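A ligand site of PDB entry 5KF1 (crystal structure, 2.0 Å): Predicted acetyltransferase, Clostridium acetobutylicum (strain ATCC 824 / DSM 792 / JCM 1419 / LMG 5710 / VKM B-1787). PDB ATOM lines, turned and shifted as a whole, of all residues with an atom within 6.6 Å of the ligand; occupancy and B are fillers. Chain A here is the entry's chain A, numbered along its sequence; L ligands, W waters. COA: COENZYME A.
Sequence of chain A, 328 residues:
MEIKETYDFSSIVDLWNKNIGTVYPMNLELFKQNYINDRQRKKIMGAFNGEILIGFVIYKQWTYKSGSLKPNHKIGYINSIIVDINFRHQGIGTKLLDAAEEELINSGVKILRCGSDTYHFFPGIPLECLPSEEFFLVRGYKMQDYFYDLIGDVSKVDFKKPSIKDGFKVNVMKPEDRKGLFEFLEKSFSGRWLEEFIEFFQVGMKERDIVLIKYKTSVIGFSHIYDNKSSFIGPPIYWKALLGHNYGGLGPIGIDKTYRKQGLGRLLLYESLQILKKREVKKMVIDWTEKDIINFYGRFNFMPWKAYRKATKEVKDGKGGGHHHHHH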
ATOM      1  N   PHE A 189      21.529  -3.579 -13.812  1.00  0.00           N
ATOM      2  CA  PHE A 189      22.799  -4.117 -14.288  1.00  0.00           C
ATOM      3  C   PHE A 189      23.230  -5.374 -13.562  1.00  0.00           C
ATOM      4  O   PHE A 189      24.300  -5.404 -12.958  1.00  0.00           O
ATOM      5  CB  PHE A 189      23.883  -3.051 -14.152  1.00  0.00           C
ATOM      6  CG  PHE A 189      23.788  -1.941 -15.155  1.00  0.00           C
ATOM      7  CD1 PHE A 189      23.878  -2.215 -16.518  1.00  0.00           C
ATOM      8  CD2 PHE A 189      23.660  -0.626 -14.745  1.00  0.00           C
ATOM      9  CE1 PHE A 189      23.800  -1.206 -17.452  1.00  0.00           C
ATOM     10  CE2 PHE A 189      23.599   0.394 -15.679  1.00  0.00           C
ATOM     11  CZ  PHE A 189      23.663   0.105 -17.042  1.00  0.00           C
ATOM     12  N   TRP A 193      28.327  -6.504 -14.304  1.00  0.00           N
ATOM     13  CA  TRP A 193      28.690  -5.314 -13.568  1.00  0.00           C
ATOM     14  C   TRP A 193      28.267  -5.392 -12.118  1.00  0.00           C
ATOM     15  O   TRP A 193      28.959  -4.881 -11.250  1.00  0.00           O
ATOM     16  CB  TRP A 193      28.185  -4.035 -14.227  1.00  0.00           C
ATOM     17  CG  TRP A 193      28.891  -3.737 -15.486  1.00  0.00           C
ATOM     18  CD1 TRP A 193      30.034  -4.335 -15.957  1.00  0.00           C
ATOM     19  CD2 TRP A 193      28.536  -2.759 -16.437  1.00  0.00           C
ATOM     20  NE1 TRP A 193      30.392  -3.793 -17.151  1.00  0.00           N
ATOM     21  CE2 TRP A 193      29.495  -2.819 -17.477  1.00  0.00           C
ATOM     22  CE3 TRP A 193      27.503  -1.820 -16.508  1.00  0.00           C
ATOM     23  CZ2 TRP A 193      29.443  -1.994 -18.580  1.00  0.00           C
ATOM     24  CZ3 TRP A 193      27.448  -0.990 -17.597  1.00  0.00           C
ATOM     25  CH2 TRP A 193      28.431  -1.070 -18.618  1.00  0.00           C
ATOM     26  N   PRO A 252      33.737   0.645 -16.039  1.00  0.00           N
ATOM     27  CA  PRO A 252      32.581   0.999 -16.866  1.00  0.00           C
ATOM     28  C   PRO A 252      31.814   2.233 -16.477  1.00  0.00           C
ATOM     29  O   PRO A 252      32.139   2.926 -15.520  1.00  0.00           O
ATOM     30  CB  PRO A 252      31.670  -0.212 -16.744  1.00  0.00           C
ATOM     31  CG  PRO A 252      32.093  -0.914 -15.505  1.00  0.00           C
ATOM     32  CD  PRO A 252      33.574  -0.648 -15.371  1.00  0.00           C
ATOM     33  N   ILE A 253      30.788   2.495 -17.257  1.00  0.00           N
ATOM     34  CA  ILE A 253      29.904   3.602 -17.029  1.00  0.00           C
ATOM     35  C   ILE A 253      28.541   3.162 -17.543  1.00  0.00           C
ATOM     36  O   ILE A 253      28.427   2.496 -18.590  1.00  0.00           O
ATOM     37  CB  ILE A 253      30.441   4.870 -17.755  1.00  0.00           C
ATOM     38  CG1 ILE A 253      29.444   6.008 -17.632  1.00  0.00           C
ATOM     39  CG2 ILE A 253      30.678   4.612 -19.241  1.00  0.00           C
ATOM     40  CD1 ILE A 253      30.060   7.313 -18.069  1.00  0.00           C
ATOM     41  N   GLY A 254      27.496   3.510 -16.804  1.00  0.00           N
ATOM     42  CA  GLY A 254      26.155   2.994 -17.111  1.00  0.00           C
ATOM     43  C   GLY A 254      25.063   3.844 -16.507  1.00  0.00           C
ATOM     44  O   GLY A 254      25.176   4.307 -15.392  1.00  0.00           O
ATOM     45  N   ILE A 255      24.012   4.070 -17.273  1.00  0.00           N
ATOM     46  CA  ILE A 255      22.854   4.859 -16.894  1.00  0.00           C
ATOM     47  C   ILE A 255      21.705   3.857 -16.961  1.00  0.00           C
ATOM     48  O   ILE A 255      21.586   3.067 -17.921  1.00  0.00           O
ATOM     49  CB  ILE A 255      22.663   6.028 -17.909  1.00  0.00           C
ATOM     50  CG1 ILE A 255      23.649   7.168 -17.661  1.00  0.00           C
ATOM     51  CG2 ILE A 255      21.248   6.598 -17.921  1.00  0.00           C
ATOM     52  CD1 ILE A 255      23.705   7.714 -16.265  1.00  0.00           C
ATOM     53  N   ASP A 256      20.861   3.868 -15.930  1.00  0.00           N
ATOM     54  CA  ASP A 256      19.621   3.079 -15.945  1.00  0.00           C
ATOM     55  C   ASP A 256      18.995   3.122 -17.322  1.00  0.00           C
ATOM     56  O   ASP A 256      18.935   4.187 -17.904  1.00  0.00           O
ATOM     57  CB  ASP A 256      18.592   3.674 -14.980  1.00  0.00           C
ATOM     58  CG  ASP A 256      17.335   2.873 -14.941  1.00  0.00           C
ATOM     59  OD1 ASP A 256      16.349   3.254 -15.622  1.00  0.00           O
ATOM     60  OD2 ASP A 256      17.386   1.818 -14.288  1.00  0.00           O
ATOM     61  N   LYS A 257      18.455   1.995 -17.792  1.00  0.00           N
ATOM     62  CA  LYS A 257      17.842   1.980 -19.139  1.00  0.00           C
ATOM     63  C   LYS A 257      16.759   3.021 -19.455  1.00  0.00           C
ATOM     64  O   LYS A 257      16.747   3.562 -20.559  1.00  0.00           O
ATOM     65  CB  LYS A 257      17.305   0.588 -19.465  1.00  0.00           C
ATOM     66  CG  LYS A 257      17.301   0.297 -20.966  1.00  0.00           C
ATOM     67  CD  LYS A 257      16.020   0.731 -21.673  1.00  0.00           C
ATOM     68  CE  LYS A 257      15.250  -0.480 -22.199  1.00  0.00           C
ATOM     69  NZ  LYS A 257      15.932  -1.179 -23.332  1.00  0.00           N
ATOM     70  N   TYR A 259      16.478   5.994 -18.312  1.00  0.00           N
ATOM     71  CA  TYR A 259      17.053   7.317 -18.343  1.00  0.00           C
ATOM     72  C   TYR A 259      18.015   7.605 -19.509  1.00  0.00           C
ATOM     73  O   TYR A 259      18.593   8.684 -19.541  1.00  0.00           O
ATOM     74  CB  TYR A 259      17.766   7.565 -17.022  1.00  0.00           C
ATOM     75  CG  TYR A 259      16.809   7.841 -15.894  1.00  0.00           C
ATOM     76  CD1 TYR A 259      16.177   9.078 -15.804  1.00  0.00           C
ATOM     77  CD2 TYR A 259      16.543   6.885 -14.920  1.00  0.00           C
ATOM     78  CE1 TYR A 259      15.315   9.356 -14.761  1.00  0.00           C
ATOM     79  CE2 TYR A 259      15.671   7.161 -13.887  1.00  0.00           C
ATOM     80  CZ  TYR A 259      15.063   8.397 -13.814  1.00  0.00           C
ATOM     81  OH  TYR A 259      14.200   8.677 -12.780  1.00  0.00           O
ATOM     82  N   ARG A 260      18.183   6.702 -20.463  1.00  0.00           N
ATOM     83  CA  ARG A 260      19.204   6.933 -21.511  1.00  0.00           C
ATOM     84  C   ARG A 260      18.751   7.900 -22.596  1.00  0.00           C
ATOM     85  O   ARG A 260      17.594   8.310 -22.623  1.00  0.00           O
ATOM     86  CB  ARG A 260      19.641   5.607 -22.121  1.00  0.00           C
ATOM     87  CG  ARG A 260      20.351   4.722 -21.127  1.00  0.00           C
ATOM     88  CD  ARG A 260      20.680   3.320 -21.622  1.00  0.00           C
ATOM     89  NE  ARG A 260      21.022   2.450 -20.490  1.00  0.00           N
ATOM     90  CZ  ARG A 260      21.162   1.128 -20.536  1.00  0.00           C
ATOM     91  NH1 ARG A 260      21.031   0.471 -21.674  1.00  0.00           N
ATOM     92  NH2 ARG A 260      21.464   0.469 -19.439  1.00  0.00           N
ATOM     93  N   LYS A 261      19.683   8.284 -23.472  1.00  0.00           N
ATOM     94  CA  LYS A 261      19.370   9.128 -24.642  1.00  0.00           C
ATOM     95  C   LYS A 261      18.741  10.483 -24.316  1.00  0.00           C
ATOM     96  O   LYS A 261      18.015  11.036 -25.132  1.00  0.00           O
ATOM     97  CB  LYS A 261      18.476   8.359 -25.623  1.00  0.00           C
ATOM     98  CG  LYS A 261      18.969   6.958 -25.980  1.00  0.00           C
ATOM     99  CD  LYS A 261      20.406   6.901 -26.504  1.00  0.00           C
ATOM    100  CE  LYS A 261      20.678   7.798 -27.716  1.00  0.00           C
ATOM    101  NZ  LYS A 261      20.148   7.266 -29.005  1.00  0.00           N
ATOM    102  N   GLN A 262      19.035  11.015 -23.127  1.00  0.00           N
ATOM    103  CA  GLN A 262      18.639  12.357 -22.704  1.00  0.00           C
ATOM    104  C   GLN A 262      19.843  13.152 -22.203  1.00  0.00           C
ATOM    105  O   GLN A 262      19.646  14.086 -21.427  1.00  0.00           O
ATOM    106  CB  GLN A 262      17.673  12.313 -21.515  1.00  0.00           C
ATOM    107  CG  GLN A 262      16.514  11.344 -21.557  1.00  0.00           C
ATOM    108  CD  GLN A 262      15.980  11.031 -20.145  1.00  0.00           C
ATOM    109  OE1 GLN A 262      15.995  11.892 -19.256  1.00  0.00           O
ATOM    110  NE2 GLN A 262      15.536   9.797 -19.938  1.00  0.00           N
ATOM    111  N   GLY A 263      21.078  12.777 -22.559  1.00  0.00           N
ATOM    112  CA  GLY A 263      22.257  13.560 -22.144  1.00  0.00           C
ATOM    113  C   GLY A 263      22.813  13.221 -20.760  1.00  0.00           C
ATOM    114  O   GLY A 263      23.772  13.845 -20.288  1.00  0.00           O
ATOM    115  N   LEU A 264      22.256  12.242 -20.068  1.00  0.00           N
ATOM    116  CA  LEU A 264      22.681  12.032 -18.696  1.00  0.00           C
ATOM    117  C   LEU A 264      24.040  11.307 -18.630  1.00  0.00           C
ATOM    118  O   LEU A 264      24.883  11.622 -17.767  1.00  0.00           O
ATOM    119  CB  LEU A 264      21.596  11.334 -17.910  1.00  0.00           C
ATOM    120  CG  LEU A 264      20.304  12.171 -17.777  1.00  0.00           C
ATOM    121  CD1 LEU A 264      19.220  11.399 -17.050  1.00  0.00           C
ATOM    122  CD2 LEU A 264      20.564  13.523 -17.113  1.00  0.00           C
ATOM    123  N   GLY A 265      24.277  10.371 -19.557  1.00  0.00           N
ATOM    124  CA  GLY A 265      25.633   9.784 -19.668  1.00  0.00           C
ATOM    125  C   GLY A 265      26.682  10.858 -19.955  1.00  0.00           C
ATOM    126  O   GLY A 265      27.794  10.892 -19.370  1.00  0.00           O
ATOM    127  N   ARG A 266      26.324  11.765 -20.844  1.00  0.00           N
ATOM    128  CA  ARG A 266      27.219  12.858 -21.166  1.00  0.00           C
ATOM    129  C   ARG A 266      27.550  13.625 -19.881  1.00  0.00           C
ATOM    130  O   ARG A 266      28.730  13.911 -19.610  1.00  0.00           O
ATOM    131  CB  ARG A 266      26.634  13.716 -22.305  1.00  0.00           C
ATOM    132  CG  ARG A 266      27.289  15.068 -22.527  1.00  0.00           C
ATOM    133  CD  ARG A 266      28.047  15.140 -23.835  1.00  0.00           C
ATOM    134  NE  ARG A 266      27.218  14.996 -25.051  1.00  0.00           N
ATOM    135  CZ  ARG A 266      27.602  14.372 -26.179  1.00  0.00           C
ATOM    136  NH1 ARG A 266      28.806  13.799 -26.307  1.00  0.00           N
ATOM    137  NH2 ARG A 266      26.755  14.324 -27.195  1.00  0.00           N
ATOM    138  N   LEU A 267      26.545  13.909 -19.065  1.00  0.00           N
ATOM    139  CA  LEU A 267      26.762  14.631 -17.814  1.00  0.00           C
ATOM    140  C   LEU A 267      27.589  13.826 -16.827  1.00  0.00           C
ATOM    141  O   LEU A 267      28.512  14.355 -16.209  1.00  0.00           O
ATOM    142  CB  LEU A 267      25.433  14.980 -17.165  1.00  0.00           C
ATOM    143  CG  LEU A 267      25.489  15.617 -15.769  1.00  0.00           C
ATOM    144  CD1 LEU A 267      26.313  16.887 -15.786  1.00  0.00           C
ATOM    145  CD2 LEU A 267      24.065  15.932 -15.306  1.00  0.00           C
ATOM    146  N   LEU A 268      27.273  12.541 -16.687  1.00  0.00           N
ATOM    147  CA  LEU A 268      28.056  11.677 -15.820  1.00  0.00           C
ATOM    148  C   LEU A 268      29.536  11.607 -16.261  1.00  0.00           C
ATOM    149  O   LEU A 268      30.482  11.634 -15.437  1.00  0.00           O
ATOM    150  CB  LEU A 268      27.415  10.291 -15.798  1.00  0.00           C
ATOM    151  CG  LEU A 268      28.179   9.200 -15.073  1.00  0.00           C
ATOM    152  CD1 LEU A 268      28.450   9.465 -13.585  1.00  0.00           C
ATOM    153  CD2 LEU A 268      27.411   7.923 -15.255  1.00  0.00           C
ATOM    154  N   GLU A 290      33.068  -0.146 -27.996  1.00  0.00           N
ATOM    155  CA  GLU A 290      32.635  -0.495 -29.371  1.00  0.00           C
ATOM    156  C   GLU A 290      32.766   0.689 -30.331  1.00  0.00           C
ATOM    157  O   GLU A 290      32.702   1.849 -29.914  1.00  0.00           O
ATOM    158  CB  GLU A 290      31.161  -0.904 -29.340  1.00  0.00           C
ATOM    159  CG  GLU A 290      30.963  -2.306 -28.834  1.00  0.00           C
ATOM    160  CD  GLU A 290      29.512  -2.733 -28.760  1.00  0.00           C
ATOM    161  OE1 GLU A 290      28.618  -1.848 -28.696  1.00  0.00           O
ATOM    162  OE2 GLU A 290      29.267  -3.959 -28.776  1.00  0.00           O
ATOM    163  N   ILE A 293      30.212   3.681 -30.024  1.00  0.00           N
ATOM    164  CA  ILE A 293      30.255   4.584 -28.845  1.00  0.00           C
ATOM    165  C   ILE A 293      31.532   5.425 -28.755  1.00  0.00           C
ATOM    166  O   ILE A 293      31.611   6.317 -27.923  1.00  0.00           O
ATOM    167  CB  ILE A 293      30.047   3.769 -27.531  1.00  0.00           C
ATOM    168  CG1 ILE A 293      29.478   4.643 -26.392  1.00  0.00           C
ATOM    169  CG2 ILE A 293      31.310   3.074 -27.076  1.00  0.00           C
ATOM    170  CD1 ILE A 293      28.022   5.079 -26.606  1.00  0.00           C
ATOM    171  N   PHE A 296      31.170   9.337 -28.462  1.00  0.00           N
ATOM    172  CA  PHE A 296      30.642   9.755 -27.159  1.00  0.00           C
ATOM    173  C   PHE A 296      31.815  10.169 -26.322  1.00  0.00           C
ATOM    174  O   PHE A 296      31.773  11.216 -25.701  1.00  0.00           O
ATOM    175  CB  PHE A 296      29.903   8.580 -26.520  1.00  0.00           C
ATOM    176  CG  PHE A 296      29.498   8.788 -25.102  1.00  0.00           C
ATOM    177  CD1 PHE A 296      28.620   9.828 -24.759  1.00  0.00           C
ATOM    178  CD2 PHE A 296      29.904   7.897 -24.132  1.00  0.00           C
ATOM    179  CE1 PHE A 296      28.219   9.994 -23.432  1.00  0.00           C
ATOM    180  CE2 PHE A 296      29.489   8.049 -22.796  1.00  0.00           C
ATOM    181  CZ  PHE A 296      28.646   9.108 -22.443  1.00  0.00           C
ATOM    182  N   TYR A 297      32.873   9.360 -26.351  1.00  0.00           N
ATOM    183  CA  TYR A 297      34.083   9.738 -25.653  1.00  0.00           C
ATOM    184  C   TYR A 297      34.949  10.702 -26.481  1.00  0.00           C
ATOM    185  O   TYR A 297      35.677  11.516 -25.914  1.00  0.00           O
ATOM    186  CB  TYR A 297      34.860   8.507 -25.306  1.00  0.00           C
ATOM    187  CG  TYR A 297      34.090   7.504 -24.480  1.00  0.00           C
ATOM    188  CD1 TYR A 297      33.798   7.761 -23.144  1.00  0.00           C
ATOM    189  CD2 TYR A 297      33.632   6.309 -25.046  1.00  0.00           C
ATOM    190  CE1 TYR A 297      33.131   6.840 -22.376  1.00  0.00           C
ATOM    191  CE2 TYR A 297      32.946   5.381 -24.287  1.00  0.00           C
ATOM    192  CZ  TYR A 297      32.695   5.647 -22.968  1.00  0.00           C
ATOM    193  OH  TYR A 297      32.037   4.751 -22.236  1.00  0.00           O
HETATM  194  O5B COA L   1      22.177  10.548 -23.710  1.00  0.00           O
HETATM  195  P1A COA L   1      23.682  10.521 -23.708  1.00  0.00           P
HETATM  196  O1A COA L   1      24.318  10.492 -25.210  1.00  0.00           O
HETATM  197  O2A COA L   1      24.492  11.404 -22.809  1.00  0.00           O
HETATM  198  O3A COA L   1      24.064   8.999 -23.348  1.00  0.00           O
HETATM  199  P2A COA L   1      23.183   8.001 -22.496  1.00  0.00           P
HETATM  200  O4A COA L   1      22.404   7.165 -23.450  1.00  0.00           O
HETATM  201  O5A COA L   1      22.528   8.695 -21.316  1.00  0.00           O
HETATM  202  O6A COA L   1      24.347   7.124 -21.857  1.00  0.00           O
HETATM  203  CBP COA L   1      25.540   5.055 -21.931  1.00  0.00           C
HETATM  204  CCP COA L   1      25.300   6.383 -22.629  1.00  0.00           C
HETATM  205  CDP COA L   1      26.517   4.205 -22.737  1.00  0.00           C
HETATM  206  CEP COA L   1      26.166   5.289 -20.541  1.00  0.00           C
HETATM  207  CAP COA L   1      24.181   4.354 -21.812  1.00  0.00           C
HETATM  208  OAP COA L   1      23.606   4.244 -23.125  1.00  0.00           O
HETATM  209  C9P COA L   1      24.371   3.048 -21.095  1.00  0.00           C
HETATM  210  O9P COA L   1      24.287   3.020 -19.874  1.00  0.00           O
HETATM  211  N8P COA L   1      24.688   1.964 -21.777  1.00  0.00           N
HETATM  212  C7P COA L   1      25.035   0.727 -21.069  1.00  0.00           C
HETATM  213  C6P COA L   1      26.119  -0.128 -21.673  1.00  0.00           C
HETATM  214  C5P COA L   1      27.380   0.567 -22.173  1.00  0.00           C
HETATM  215  O5P COA L   1      27.652   0.321 -23.349  1.00  0.00           O
HETATM  216  N4P COA L   1      28.199   1.326 -21.374  1.00  0.00           N
HETATM  217  O   HOH W   1      31.300   1.012 -20.107  1.00  0.00           O
HETATM  218  O   HOH W   2      20.562  10.251 -20.706  1.00  0.00           O
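The backbone NH of Lys 261 lies within hydrogen-bond range of an oxygen (O4A) of the ligand, at 2.9 Å. The backbone NH (N) of Gln 262 lies within hydrogen-bond range of an oxygen (O5B) of the ligand (3.2 Å). N of Gly 263 is in hydrogen-bond range of O5B of the ligand. N4P of the ligand is in hydrogen-bond range of O of Ile 253, at 3.0 Å. O5A of the ligand sits at hydrogen-bond distance from N of Gly 265. The backbone NH of Arg 266 is in hydrogen-bond range of an oxygen (O2A) of the ligand (2.7 Å). An oxygen (O9P) of the ligand is in hydrogen-bond range of the backbone NH (N) of Ile 255 (2.8 Å). NE of Arg 260 lies within hydrogen-bond range of O9P of the ligand, 3.4 Å away.
O of Tyr 259 sits at hydrogen-bond distance from NE2 of Gln 262, at 3.3 Å. The guanidinium group of Arg 260 is in hydrogen-bond range of the backbone carbonyl oxygen of Ile 255 (2.7 Å).
Residues that only touch the ligand: Gly 254, Leu 264 and Trp 193. Hydrophobic or aromatic side chains that line the ligand: Trp 193 and Ile 255. 11 residues have an atom within 4 Å of the ligand: Trp 193, Ile 253, Gly 254, Ile 255, Arg 260, Lys 261, Gln 262, Gly 263, Leu 264, Gly 265 and Arg 266.
Water W1 bridges N of Ile 253 and N4P of the ligand.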
